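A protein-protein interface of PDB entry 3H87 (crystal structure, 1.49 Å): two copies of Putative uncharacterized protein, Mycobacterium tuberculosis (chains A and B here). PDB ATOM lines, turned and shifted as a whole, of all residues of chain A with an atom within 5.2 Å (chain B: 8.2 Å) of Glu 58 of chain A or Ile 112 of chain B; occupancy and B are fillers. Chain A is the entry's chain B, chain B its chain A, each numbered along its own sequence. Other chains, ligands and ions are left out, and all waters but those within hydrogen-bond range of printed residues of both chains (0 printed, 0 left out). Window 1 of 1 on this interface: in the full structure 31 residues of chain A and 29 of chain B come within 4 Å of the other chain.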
ATOM      1  N   LYS A  25      36.132   9.193  24.905  1.00  0.00           N
ATOM      2  CA  LYS A  25      35.800   8.348  23.756  1.00  0.00           C
ATOM      3  C   LYS A  25      36.519   8.746  22.484  1.00  0.00           C
ATOM      4  O   LYS A  25      36.865   7.873  21.648  1.00  0.00           O
ATOM      5  CB  LYS A  25      34.283   8.303  23.482  1.00  0.00           C
ATOM      6  CG  LYS A  25      33.613   9.687  23.163  1.00  0.00           C
ATOM      7  CD  LYS A  25      32.180   9.509  22.714  1.00  0.00           C
ATOM      8  CE  LYS A  25      31.446  10.835  22.489  1.00  0.00           C
ATOM      9  NZ  LYS A  25      31.198  11.550  23.809  1.00  0.00           N
ATOM     10  N   VAL A  54      30.697   6.734  32.633  1.00  0.00           N
ATOM     11  CA  VAL A  54      29.958   7.265  31.489  1.00  0.00           C
ATOM     12  C   VAL A  54      30.585   6.820  30.161  1.00  0.00           C
ATOM     13  O   VAL A  54      29.862   6.416  29.221  1.00  0.00           O
ATOM     14  CB  VAL A  54      29.935   8.824  31.577  1.00  0.00           C
ATOM     15  CG1 VAL A  54      29.497   9.499  30.246  1.00  0.00           C
ATOM     16  CG2 VAL A  54      29.002   9.225  32.776  1.00  0.00           C
ATOM     17  N   THR A  55      31.913   6.888  30.030  1.00  0.00           N
ATOM     18  CA  THR A  55      32.575   6.445  28.780  1.00  0.00           C
ATOM     19  C   THR A  55      32.380   4.930  28.556  1.00  0.00           C
ATOM     20  O   THR A  55      32.214   4.487  27.425  1.00  0.00           O
ATOM     21  CB  THR A  55      34.071   6.834  28.774  1.00  0.00           C
ATOM     22  OG1 THR A  55      34.173   8.263  29.008  1.00  0.00           O
ATOM     23  CG2 THR A  55      34.773   6.470  27.460  1.00  0.00           C
ATOM     24  N   ARG A  56      32.313   4.129  29.617  1.00  0.00           N
ATOM     25  CA  ARG A  56      32.045   2.704  29.505  1.00  0.00           C
ATOM     26  C   ARG A  56      30.643   2.512  28.904  1.00  0.00           C
ATOM     27  O   ARG A  56      30.428   1.595  28.058  1.00  0.00           O
ATOM     28  CB  ARG A  56      32.257   1.992  30.860  1.00  0.00           C
ATOM     29  CG  ARG A  56      33.730   1.922  31.239  1.00  0.00           C
ATOM     30  CD  ARG A  56      34.025   1.591  32.719  1.00  0.00           C
ATOM     31  NE  ARG A  56      33.387   0.388  33.158  1.00  0.00           N
ATOM     32  CZ  ARG A  56      33.904  -0.833  32.986  1.00  0.00           C
ATOM     33  NH1 ARG A  56      35.111  -1.046  32.459  1.00  0.00           N
ATOM     34  NH2 ARG A  56      33.233  -1.902  33.344  1.00  0.00           N
ATOM     35  N   LEU A  57      29.644   3.297  29.326  1.00  0.00           N
ATOM     36  CA  LEU A  57      28.309   3.233  28.719  1.00  0.00           C
ATOM     37  C   LEU A  57      28.317   3.605  27.231  1.00  0.00           C
ATOM     38  O   LEU A  57      27.530   3.086  26.432  1.00  0.00           O
ATOM     39  CB  LEU A  57      27.301   4.069  29.521  1.00  0.00           C
ATOM     40  CG  LEU A  57      26.768   3.421  30.780  1.00  0.00           C
ATOM     41  CD1 LEU A  57      26.312   4.454  31.837  1.00  0.00           C
ATOM     42  CD2 LEU A  57      25.637   2.450  30.409  1.00  0.00           C
ATOM     43  N   GLU A  58      29.180   4.561  26.869  1.00  0.00           N
ATOM     44  CA  GLU A  58      29.343   4.922  25.447  1.00  0.00           C
ATOM     45  C   GLU A  58      29.955   3.746  24.641  1.00  0.00           C
ATOM     46  O   GLU A  58      29.519   3.444  23.524  1.00  0.00           O
ATOM     47  CB  GLU A  58      30.174   6.208  25.279  1.00  0.00           C
ATOM     48  CG  GLU A  58      29.472   7.432  25.887  1.00  0.00           C
ATOM     49  CD  GLU A  58      30.289   8.698  25.726  1.00  0.00           C
ATOM     50  OE1 GLU A  58      31.522   8.602  26.002  1.00  0.00           O
ATOM     51  OE2 GLU A  58      29.726   9.717  25.280  1.00  0.00           O
ATOM     52  N   VAL A  59      30.965   3.087  25.205  1.00  0.00           N
ATOM     53  CA  VAL A  59      31.514   1.841  24.614  1.00  0.00           C
ATOM     54  C   VAL A  59      30.404   0.808  24.406  1.00  0.00           C
ATOM     55  O   VAL A  59      30.270   0.233  23.317  1.00  0.00           O
ATOM     56  CB  VAL A  59      32.621   1.282  25.485  1.00  0.00           C
ATOM     57  CG1 VAL A  59      32.993  -0.169  25.088  1.00  0.00           C
ATOM     58  CG2 VAL A  59      33.845   2.194  25.439  1.00  0.00           C
ATOM     59  N   GLY A  60      29.551   0.581  25.399  1.00  0.00           N
ATOM     60  CA  GLY A  60      28.471  -0.407  25.266  1.00  0.00           C
ATOM     61  C   GLY A  60      27.485  -0.021  24.187  1.00  0.00           C
ATOM     62  O   GLY A  60      26.972  -0.859  23.447  1.00  0.00           O
ATOM     63  N   PHE A  61      27.159   1.277  24.106  1.00  0.00           N
ATOM     64  CA  PHE A  61      26.216   1.758  23.080  1.00  0.00           C
ATOM     65  C   PHE A  61      26.769   1.489  21.680  1.00  0.00           C
ATOM     66  O   PHE A  61      26.035   1.102  20.741  1.00  0.00           O
ATOM     67  CB  PHE A  61      25.916   3.288  23.246  1.00  0.00           C
ATOM     68  CG  PHE A  61      24.700   3.785  22.487  1.00  0.00           C
ATOM     69  CD1 PHE A  61      23.441   3.779  23.076  1.00  0.00           C
ATOM     70  CD2 PHE A  61      24.831   4.295  21.210  1.00  0.00           C
ATOM     71  CE1 PHE A  61      22.327   4.270  22.418  1.00  0.00           C
ATOM     72  CE2 PHE A  61      23.686   4.749  20.525  1.00  0.00           C
ATOM     73  CZ  PHE A  61      22.459   4.726  21.128  1.00  0.00           C
ATOM     74  N   SER A  62      28.075   1.731  21.514  1.00  0.00           N
ATOM     75  CA  SER A  62      28.729   1.574  20.206  1.00  0.00           C
ATOM     76  C   SER A  62      28.864   0.117  19.768  1.00  0.00           C
ATOM     77  O   SER A  62      28.915  -0.166  18.564  1.00  0.00           O
ATOM     78  CB  SER A  62      30.110   2.245  20.218  1.00  0.00           C
ATOM     79  OG  SER A  62      31.096   1.504  20.917  1.00  0.00           O
ATOM     80  N   ALA A  63      28.960  -0.806  20.711  1.00  0.00           N
ATOM     81  CA  ALA A  63      29.146  -2.243  20.395  1.00  0.00           C
ATOM     82  C   ALA A  63      27.931  -2.781  19.652  1.00  0.00           C
ATOM     83  O   ALA A  63      26.799  -2.399  19.965  1.00  0.00           O
ATOM     84  CB  ALA A  63      29.366  -3.014  21.664  1.00  0.00           C
ATOM     85  N   PRO A 113      28.318  14.384  28.046  1.00  0.00           N
ATOM     86  CA  PRO A 113      29.476  13.565  28.425  1.00  0.00           C
ATOM     87  C   PRO A 113      30.781  14.378  28.491  1.00  0.00           C
ATOM     88  O   PRO A 113      31.625  14.138  29.376  1.00  0.00           O
ATOM     89  CB  PRO A 113      29.531  12.485  27.323  1.00  0.00           C
ATOM     90  CG  PRO A 113      28.715  12.978  26.227  1.00  0.00           C
ATOM     91  CD  PRO A 113      27.579  13.797  26.930  1.00  0.00           C
ATOM     92  N   LYS B  25      12.951  13.627  31.945  1.00  0.00           N
ATOM     93  CA  LYS B  25      12.697  14.805  31.107  1.00  0.00           C
ATOM     94  C   LYS B  25      11.397  14.750  30.310  1.00  0.00           C
ATOM     95  O   LYS B  25      10.724  15.775  30.104  1.00  0.00           O
ATOM     96  CB  LYS B  25      13.889  15.068  30.135  1.00  0.00           C
ATOM     97  CG  LYS B  25      14.169  13.926  29.098  1.00  0.00           C
ATOM     98  CD  LYS B  25      15.278  14.286  28.049  1.00  0.00           C
ATOM     99  CE  LYS B  25      15.708  13.142  27.175  1.00  0.00           C
ATOM    100  NZ  LYS B  25      16.542  12.098  27.917  1.00  0.00           N
ATOM    101  N   VAL B  54      21.839  14.130  36.084  1.00  0.00           N
ATOM    102  CA  VAL B  54      21.852  14.081  34.622  1.00  0.00           C
ATOM    103  C   VAL B  54      20.669  14.832  34.004  1.00  0.00           C
ATOM    104  O   VAL B  54      20.843  15.556  32.997  1.00  0.00           O
ATOM    105  CB  VAL B  54      21.907  12.606  34.144  1.00  0.00           C
ATOM    106  CG1 VAL B  54      21.536  12.461  32.634  1.00  0.00           C
ATOM    107  CG2 VAL B  54      23.275  12.022  34.481  1.00  0.00           C
ATOM    108  N   GLU B  58      20.411  18.063  31.323  1.00  0.00           N
ATOM    109  CA  GLU B  58      19.559  18.119  30.123  1.00  0.00           C
ATOM    110  C   GLU B  58      18.733  19.433  30.101  1.00  0.00           C
ATOM    111  O   GLU B  58      18.570  20.076  29.040  1.00  0.00           O
ATOM    112  CB  GLU B  58      18.640  16.884  30.065  1.00  0.00           C
ATOM    113  CG  GLU B  58      19.404  15.592  29.859  1.00  0.00           C
ATOM    114  CD  GLU B  58      18.493  14.411  29.857  1.00  0.00           C
ATOM    115  OE1 GLU B  58      17.600  14.341  30.730  1.00  0.00           O
ATOM    116  OE2 GLU B  58      18.619  13.608  28.915  1.00  0.00           O
ATOM    117  N   LEU B  86      24.327   9.909  41.269  1.00  0.00           N
ATOM    118  CA  LEU B  86      24.838   8.586  40.897  1.00  0.00           C
ATOM    119  C   LEU B  86      25.759   8.023  41.959  1.00  0.00           C
ATOM    120  O   LEU B  86      26.349   8.741  42.768  1.00  0.00           O
ATOM    121  CB  LEU B  86      25.554   8.627  39.532  1.00  0.00           C
ATOM    122  CG  LEU B  86      24.609   8.886  38.366  1.00  0.00           C
ATOM    123  CD1 LEU B  86      25.339   9.336  37.104  1.00  0.00           C
ATOM    124  CD2 LEU B  86      23.722   7.693  38.049  1.00  0.00           C
ATOM    125  N   ALA B  94      23.415   0.333  35.320  1.00  0.00           N
ATOM    126  CA  ALA B  94      23.051   0.850  33.988  1.00  0.00           C
ATOM    127  C   ALA B  94      23.778   0.100  32.874  1.00  0.00           C
ATOM    128  O   ALA B  94      23.208  -0.201  31.835  1.00  0.00           O
ATOM    129  CB  ALA B  94      23.298   2.395  33.893  1.00  0.00           C
ATOM    130  N   LEU B  95      25.075  -0.140  33.061  1.00  0.00           N
ATOM    131  CA  LEU B  95      25.871  -0.850  32.067  1.00  0.00           C
ATOM    132  C   LEU B  95      25.388  -2.297  31.932  1.00  0.00           C
ATOM    133  O   LEU B  95      25.332  -2.847  30.800  1.00  0.00           O
ATOM    134  CB  LEU B  95      27.385  -0.778  32.386  1.00  0.00           C
ATOM    135  CG  LEU B  95      28.367  -1.365  31.365  1.00  0.00           C
ATOM    136  CD1 LEU B  95      28.366  -0.490  30.110  1.00  0.00           C
ATOM    137  CD2 LEU B  95      29.785  -1.423  31.978  1.00  0.00           C
ATOM    138  N   GLN B  98      22.157  -2.248  29.954  1.00  0.00           N
ATOM    139  CA  GLN B  98      22.447  -1.960  28.577  1.00  0.00           C
ATOM    140  C   GLN B  98      22.894  -3.243  27.837  1.00  0.00           C
ATOM    141  O   GLN B  98      22.509  -3.506  26.693  1.00  0.00           O
ATOM    142  CB  GLN B  98      23.533  -0.902  28.466  1.00  0.00           C
ATOM    143  CG  GLN B  98      23.867  -0.480  27.041  1.00  0.00           C
ATOM    144  CD  GLN B  98      25.014   0.457  27.010  1.00  0.00           C
ATOM    145  OE1 GLN B  98      26.121   0.075  27.408  1.00  0.00           O
ATOM    146  NE2 GLN B  98      24.791   1.700  26.590  1.00  0.00           N
ATOM    147  N   HIS B 107      19.486  -2.266  22.347  1.00  0.00           N
ATOM    148  CA  HIS B 107      20.214  -1.263  23.100  1.00  0.00           C
ATOM    149  C   HIS B 107      20.457   0.103  22.455  1.00  0.00           C
ATOM    150  O   HIS B 107      21.020   0.996  23.093  1.00  0.00           O
ATOM    151  CB  HIS B 107      21.515  -1.857  23.600  1.00  0.00           C
ATOM    152  CG  HIS B 107      22.619  -1.921  22.605  1.00  0.00           C
ATOM    153  ND1 HIS B 107      22.579  -2.634  21.425  1.00  0.00           N
ATOM    154  CD2 HIS B 107      23.865  -1.391  22.697  1.00  0.00           C
ATOM    155  CE1 HIS B 107      23.762  -2.509  20.822  1.00  0.00           C
ATOM    156  NE2 HIS B 107      24.547  -1.762  21.586  1.00  0.00           N
ATOM    157  N   ARG B 108      20.022   0.296  21.218  1.00  0.00           N
ATOM    158  CA  ARG B 108      20.085   1.645  20.669  1.00  0.00           C
ATOM    159  C   ARG B 108      18.734   2.326  20.717  1.00  0.00           C
ATOM    160  O   ARG B 108      18.583   3.425  20.196  1.00  0.00           O
ATOM    161  CB  ARG B 108      20.685   1.613  19.278  1.00  0.00           C
ATOM    162  CG  ARG B 108      22.093   1.076  19.397  1.00  0.00           C
ATOM    163  CD  ARG B 108      22.956   1.458  18.307  1.00  0.00           C
ATOM    164  NE  ARG B 108      24.231   0.766  18.438  1.00  0.00           N
ATOM    165  CZ  ARG B 108      24.991   0.434  17.406  1.00  0.00           C
ATOM    166  NH1 ARG B 108      24.599   0.714  16.149  1.00  0.00           N
ATOM    167  NH2 ARG B 108      26.136  -0.179  17.615  1.00  0.00           N
ATOM    168  N   GLY B 109      17.790   1.699  21.414  1.00  0.00           N
ATOM    169  CA  GLY B 109      16.504   2.286  21.758  1.00  0.00           C
ATOM    170  C   GLY B 109      16.728   3.214  22.954  1.00  0.00           C
ATOM    171  O   GLY B 109      16.852   4.422  22.787  1.00  0.00           O
ATOM    172  N   PRO B 110      16.761   2.664  24.178  1.00  0.00           N
ATOM    173  CA  PRO B 110      17.046   3.477  25.341  1.00  0.00           C
ATOM    174  C   PRO B 110      18.399   4.185  25.315  1.00  0.00           C
ATOM    175  O   PRO B 110      19.433   3.567  25.053  1.00  0.00           O
ATOM    176  CB  PRO B 110      16.988   2.480  26.491  1.00  0.00           C
ATOM    177  CG  PRO B 110      16.137   1.341  25.972  1.00  0.00           C
ATOM    178  CD  PRO B 110      16.526   1.260  24.544  1.00  0.00           C
ATOM    179  N   SER B 111      18.377   5.472  25.582  1.00  0.00           N
ATOM    180  CA  SER B 111      19.596   6.275  25.632  1.00  0.00           C
ATOM    181  C   SER B 111      20.384   6.070  26.945  1.00  0.00           C
ATOM    182  O   SER B 111      19.898   5.427  27.891  1.00  0.00           O
ATOM    183  CB  SER B 111      19.203   7.716  25.492  1.00  0.00           C
ATOM    184  OG  SER B 111      18.470   8.121  26.640  1.00  0.00           O
ATOM    185  N   ILE B 112      21.598   6.629  26.980  1.00  0.00           N
ATOM    186  CA  ILE B 112      22.392   6.580  28.205  1.00  0.00           C
ATOM    187  C   ILE B 112      21.647   7.263  29.370  1.00  0.00           C
ATOM    188  O   ILE B 112      21.555   6.707  30.463  1.00  0.00           O
ATOM    189  CB  ILE B 112      23.862   7.029  27.942  1.00  0.00           C
ATOM    190  CG1 ILE B 112      24.534   6.069  26.968  1.00  0.00           C
ATOM    191  CG2 ILE B 112      24.627   7.123  29.281  1.00  0.00           C
ATOM    192  CD1 ILE B 112      25.936   6.488  26.505  1.00  0.00           C
ATOM    193  N   PRO B 113      21.089   8.495  29.181  1.00  0.00           N
ATOM    194  CA  PRO B 113      20.294   9.056  30.256  1.00  0.00           C
ATOM    195  C   PRO B 113      19.133   8.118  30.704  1.00  0.00           C
ATOM    196  O   PRO B 113      18.890   7.998  31.897  1.00  0.00           O
ATOM    197  CB  PRO B 113      19.799  10.414  29.684  1.00  0.00           C
ATOM    198  CG  PRO B 113      20.902  10.785  28.678  1.00  0.00           C
ATOM    199  CD  PRO B 113      21.362   9.475  28.104  1.00  0.00           C
ATOM    200  N   ASP B 114      18.422   7.476  29.765  1.00  0.00           N
ATOM    201  CA  ASP B 114      17.299   6.606  30.148  1.00  0.00           C
ATOM    202  C   ASP B 114      17.825   5.507  31.081  1.00  0.00           C
ATOM    203  O   ASP B 114      17.205   5.187  32.123  1.00  0.00           O
ATOM    204  CB  ASP B 114      16.616   5.960  28.946  1.00  0.00           C
ATOM    205  CG  ASP B 114      15.933   6.925  27.986  1.00  0.00           C
ATOM    206  OD1 ASP B 114      15.695   8.094  28.344  1.00  0.00           O
ATOM    207  OD2 ASP B 114      15.583   6.442  26.836  1.00  0.00           O
ATOM    208  N   LEU B 115      18.971   4.910  30.702  1.00  0.00           N
ATOM    209  CA  LEU B 115      19.560   3.844  31.546  1.00  0.00           C
ATOM    210  C   LEU B 115      19.958   4.340  32.942  1.00  0.00           C
ATOM    211  O   LEU B 115      19.778   3.647  33.945  1.00  0.00           O
ATOM    212  CB  LEU B 115      20.754   3.193  30.861  1.00  0.00           C
ATOM    213  CG  LEU B 115      20.416   2.407  29.615  1.00  0.00           C
ATOM    214  CD1 LEU B 115      21.689   2.275  28.724  1.00  0.00           C
ATOM    215  CD2 LEU B 115      19.873   1.030  30.008  1.00  0.00           C
ATOM    216  N   LEU B 116      20.573   5.508  32.981  1.00  0.00           N
ATOM    217  CA  LEU B 116      21.049   6.058  34.255  1.00  0.00           C
ATOM    218  C   LEU B 116      19.831   6.420  35.157  1.00  0.00           C
ATOM    219  O   LEU B 116      19.901   6.188  36.396  1.00  0.00           O
ATOM    220  CB  LEU B 116      21.960   7.282  34.012  1.00  0.00           C
ATOM    221  CG  LEU B 116      23.344   6.911  33.448  1.00  0.00           C
ATOM    222  CD1 LEU B 116      24.069   8.203  32.999  1.00  0.00           C
ATOM    223  CD2 LEU B 116      24.234   6.145  34.443  1.00  0.00           C
ATOM    224  N   ILE B 117      18.783   7.024  34.591  1.00  0.00           N
ATOM    225  CA  ILE B 117      17.564   7.355  35.391  1.00  0.00           C
ATOM    226  C   ILE B 117      16.906   6.072  35.887  1.00  0.00           C
ATOM    227  O   ILE B 117      16.538   5.957  37.054  1.00  0.00           O
ATOM    228  CB  ILE B 117      16.600   8.209  34.547  1.00  0.00           C
ATOM    229  CG1 ILE B 117      17.157   9.621  34.426  1.00  0.00           C
ATOM    230  CG2 ILE B 117      15.171   8.215  35.125  1.00  0.00           C
ATOM    231  CD1 ILE B 117      16.590  10.372  33.228  1.00  0.00           C
ATOM    232  N   ALA B 118      16.746   5.070  35.005  1.00  0.00           N
ATOM    233  CA  ALA B 118      16.109   3.845  35.441  1.00  0.00           C
ATOM    234  C   ALA B 118      16.902   3.156  36.559  1.00  0.00           C
ATOM    235  O   ALA B 118      16.318   2.660  37.531  1.00  0.00           O
ATOM    236  CB  ALA B 118      15.909   2.925  34.195  1.00  0.00           C
ATOM    237  N   ALA B 119      18.239   3.075  36.399  1.00  0.00           N
ATOM    238  CA  ALA B 119      19.035   2.380  37.450  1.00  0.00           C
ATOM    239  C   ALA B 119      19.034   3.164  38.766  1.00  0.00           C
ATOM    240  O   ALA B 119      19.060   2.580  39.861  1.00  0.00           O
ATOM    241  CB  ALA B 119      20.489   2.157  36.930  1.00  0.00           C
ATOM    242  N   PHE B 135      11.405   3.212  28.759  1.00  0.00           N
ATOM    243  CA  PHE B 135      11.358   2.751  30.167  1.00  0.00           C
ATOM    244  C   PHE B 135      10.573   1.450  30.323  1.00  0.00           C
ATOM    245  O   PHE B 135      10.906   0.648  31.194  1.00  0.00           O
ATOM    246  CB  PHE B 135      10.846   3.854  31.107  1.00  0.00           C
ATOM    247  CG  PHE B 135      11.807   4.984  31.235  1.00  0.00           C
ATOM    248  CD1 PHE B 135      12.949   4.826  31.980  1.00  0.00           C
ATOM    249  CD2 PHE B 135      11.564   6.196  30.619  1.00  0.00           C
ATOM    250  CE1 PHE B 135      13.860   5.848  32.105  1.00  0.00           C
ATOM    251  CE2 PHE B 135      12.510   7.218  30.717  1.00  0.00           C
ATOM    252  CZ  PHE B 135      13.625   7.048  31.473  1.00  0.00           C
ATOM    253  N   ILE B 138      13.198  -1.259  29.427  1.00  0.00           N
ATOM    254  CA  ILE B 138      14.070  -1.515  30.530  1.00  0.00           C
ATOM    255  C   ILE B 138      13.342  -2.310  31.641  1.00  0.00           C
ATOM    256  O   ILE B 138      13.921  -3.287  32.188  1.00  0.00           O
ATOM    257  CB  ILE B 138      14.647  -0.176  31.093  1.00  0.00           C
ATOM    258  CG1 ILE B 138      15.633   0.456  30.108  1.00  0.00           C
ATOM    259  CG2 ILE B 138      15.348  -0.425  32.439  1.00  0.00           C
ATOM    260  CD1 ILE B 138      15.984   1.943  30.417  1.00  0.00           C
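The side-chain amide nitrogen (NE2) of Gln 98 of chain B lies within hydrogen-bond range of the backbone carbonyl oxygen (O) of Leu 57 of chain A (3.1 Å).
NE2 of Gln 98 of chain B lies close to N of Phe 61 of chain A, 3.5 Å away.
The backbone carbonyl oxygen of Gly 60 of chain A lies within hydrogen-bond range of a ring nitrogen (NE2) of His 107 of chain B.
A ring nitrogen (NE2) of His 107 of chain B is in hydrogen-bond range of the backbone carbonyl oxygen (O) of Phe 61 of chain A, 3.3 Å away.
NE2 of His 107 of chain B lies within hydrogen-bond range of O of Ala 63 of chain A, 2.8 Å away.
O of Phe 61 of chain A lies within hydrogen-bond range of NE of Arg 108 of chain B, at 2.9 Å.
The guanidinium group (NH2) of Arg 108 of chain B lies within hydrogen-bond range of the backbone carbonyl oxygen (O) of Ser 62 of chain A (2.9 Å).
NH2 of Arg 108 of chain B sits at hydrogen-bond distance from O of Ala 63 of chain A.
NZ of Lys 25 of chain A lies within salt-bridge range of OE2 of Glu 58 of chain A (2.8 Å).
The side-chain hydroxyl (OG) of Ser 62 of chain A is in hydrogen-bond range of the backbone carbonyl oxygen (O) of Val 59 of chain A (2.8 Å).
Among the printed residues, merely in contact across the chains: Gly 60 of chain A with Gln 98 of chain B, Arg 56 of chain A with Leu 95 of chain B, Leu 57 of chain A with Leu 95 of chain B, Glu 58 of chain A with Ile 112 of chain B, Leu 57 of chain A with Leu 116 of chain B, Leu 57 of chain A with Ile 112 of chain B, Leu 57 of chain A with Ala 94 of chain B and Phe 61 of chain A with Pro 110 of chain B.
Glu 58 of chain A touches one residue of chain B.
Of chain A, only Leu 57 (3.8 Å) and Glu 58 (3.7 Å) come within 4 Å of Ile 112 of chain B.
Printed residues of chain A within 4 Å of Pro 110 of chain B: Phe 61 (3.98 Å).
Of the printed residues of chain A, His 107 of chain B touches Gly 60, Phe 61 and Ala 63.
Printed residues of chain A within 4 Å of Leu 116 of chain B: Leu 57.
Of the printed residues of chain A, Leu 95 of chain B touches Arg 56 and Leu 57.
Of the printed residues of chain A, Ala 94 of chain B touches Leu 57.
Leu 115 of chain B touches none of the printed residues of chain A.
The nearest printed residue of chain A that does not touch Leu 95 of chain B is Gly 60 of chain A (4.8 Å).
Of the 12 printed residues of chain A, 7 touch a printed residue of chain B.
Printed residues of chain A that touch a printed residue of chain B: Arg 56, Leu 57, Glu 58, Gly 60, Phe 61, Ser 62 and Ala 63.
Hydrophobic or aromatic side chains of chain A that line the printed part of chain B: Leu 57 and Phe 61.
Printed residues of chain B that touch a printed residue of chain A: Ala 94, Leu 95, Gln 98, His 107, Arg 108, Pro 110, Ile 112 and Leu 116.
Hydrophobic or aromatic side chains of chain B within 4 Å of the printed part of chain A: Leu 95, His 107, Ile 112 and Leu 116.
Along chain B the printed residues that touch a printed residue of chain A span positions 94 to 116.
Among the printed residues, no Asp or Glu carboxylate lies within 4 Å of a Lys or Arg side-chain nitrogen of the other chain.
Positions printed for both chains: 25, 54, 58 and 113.
Of the 16 pairs that touch across the chains among the printed residues, none has its exchanged pair printed and touching as well.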
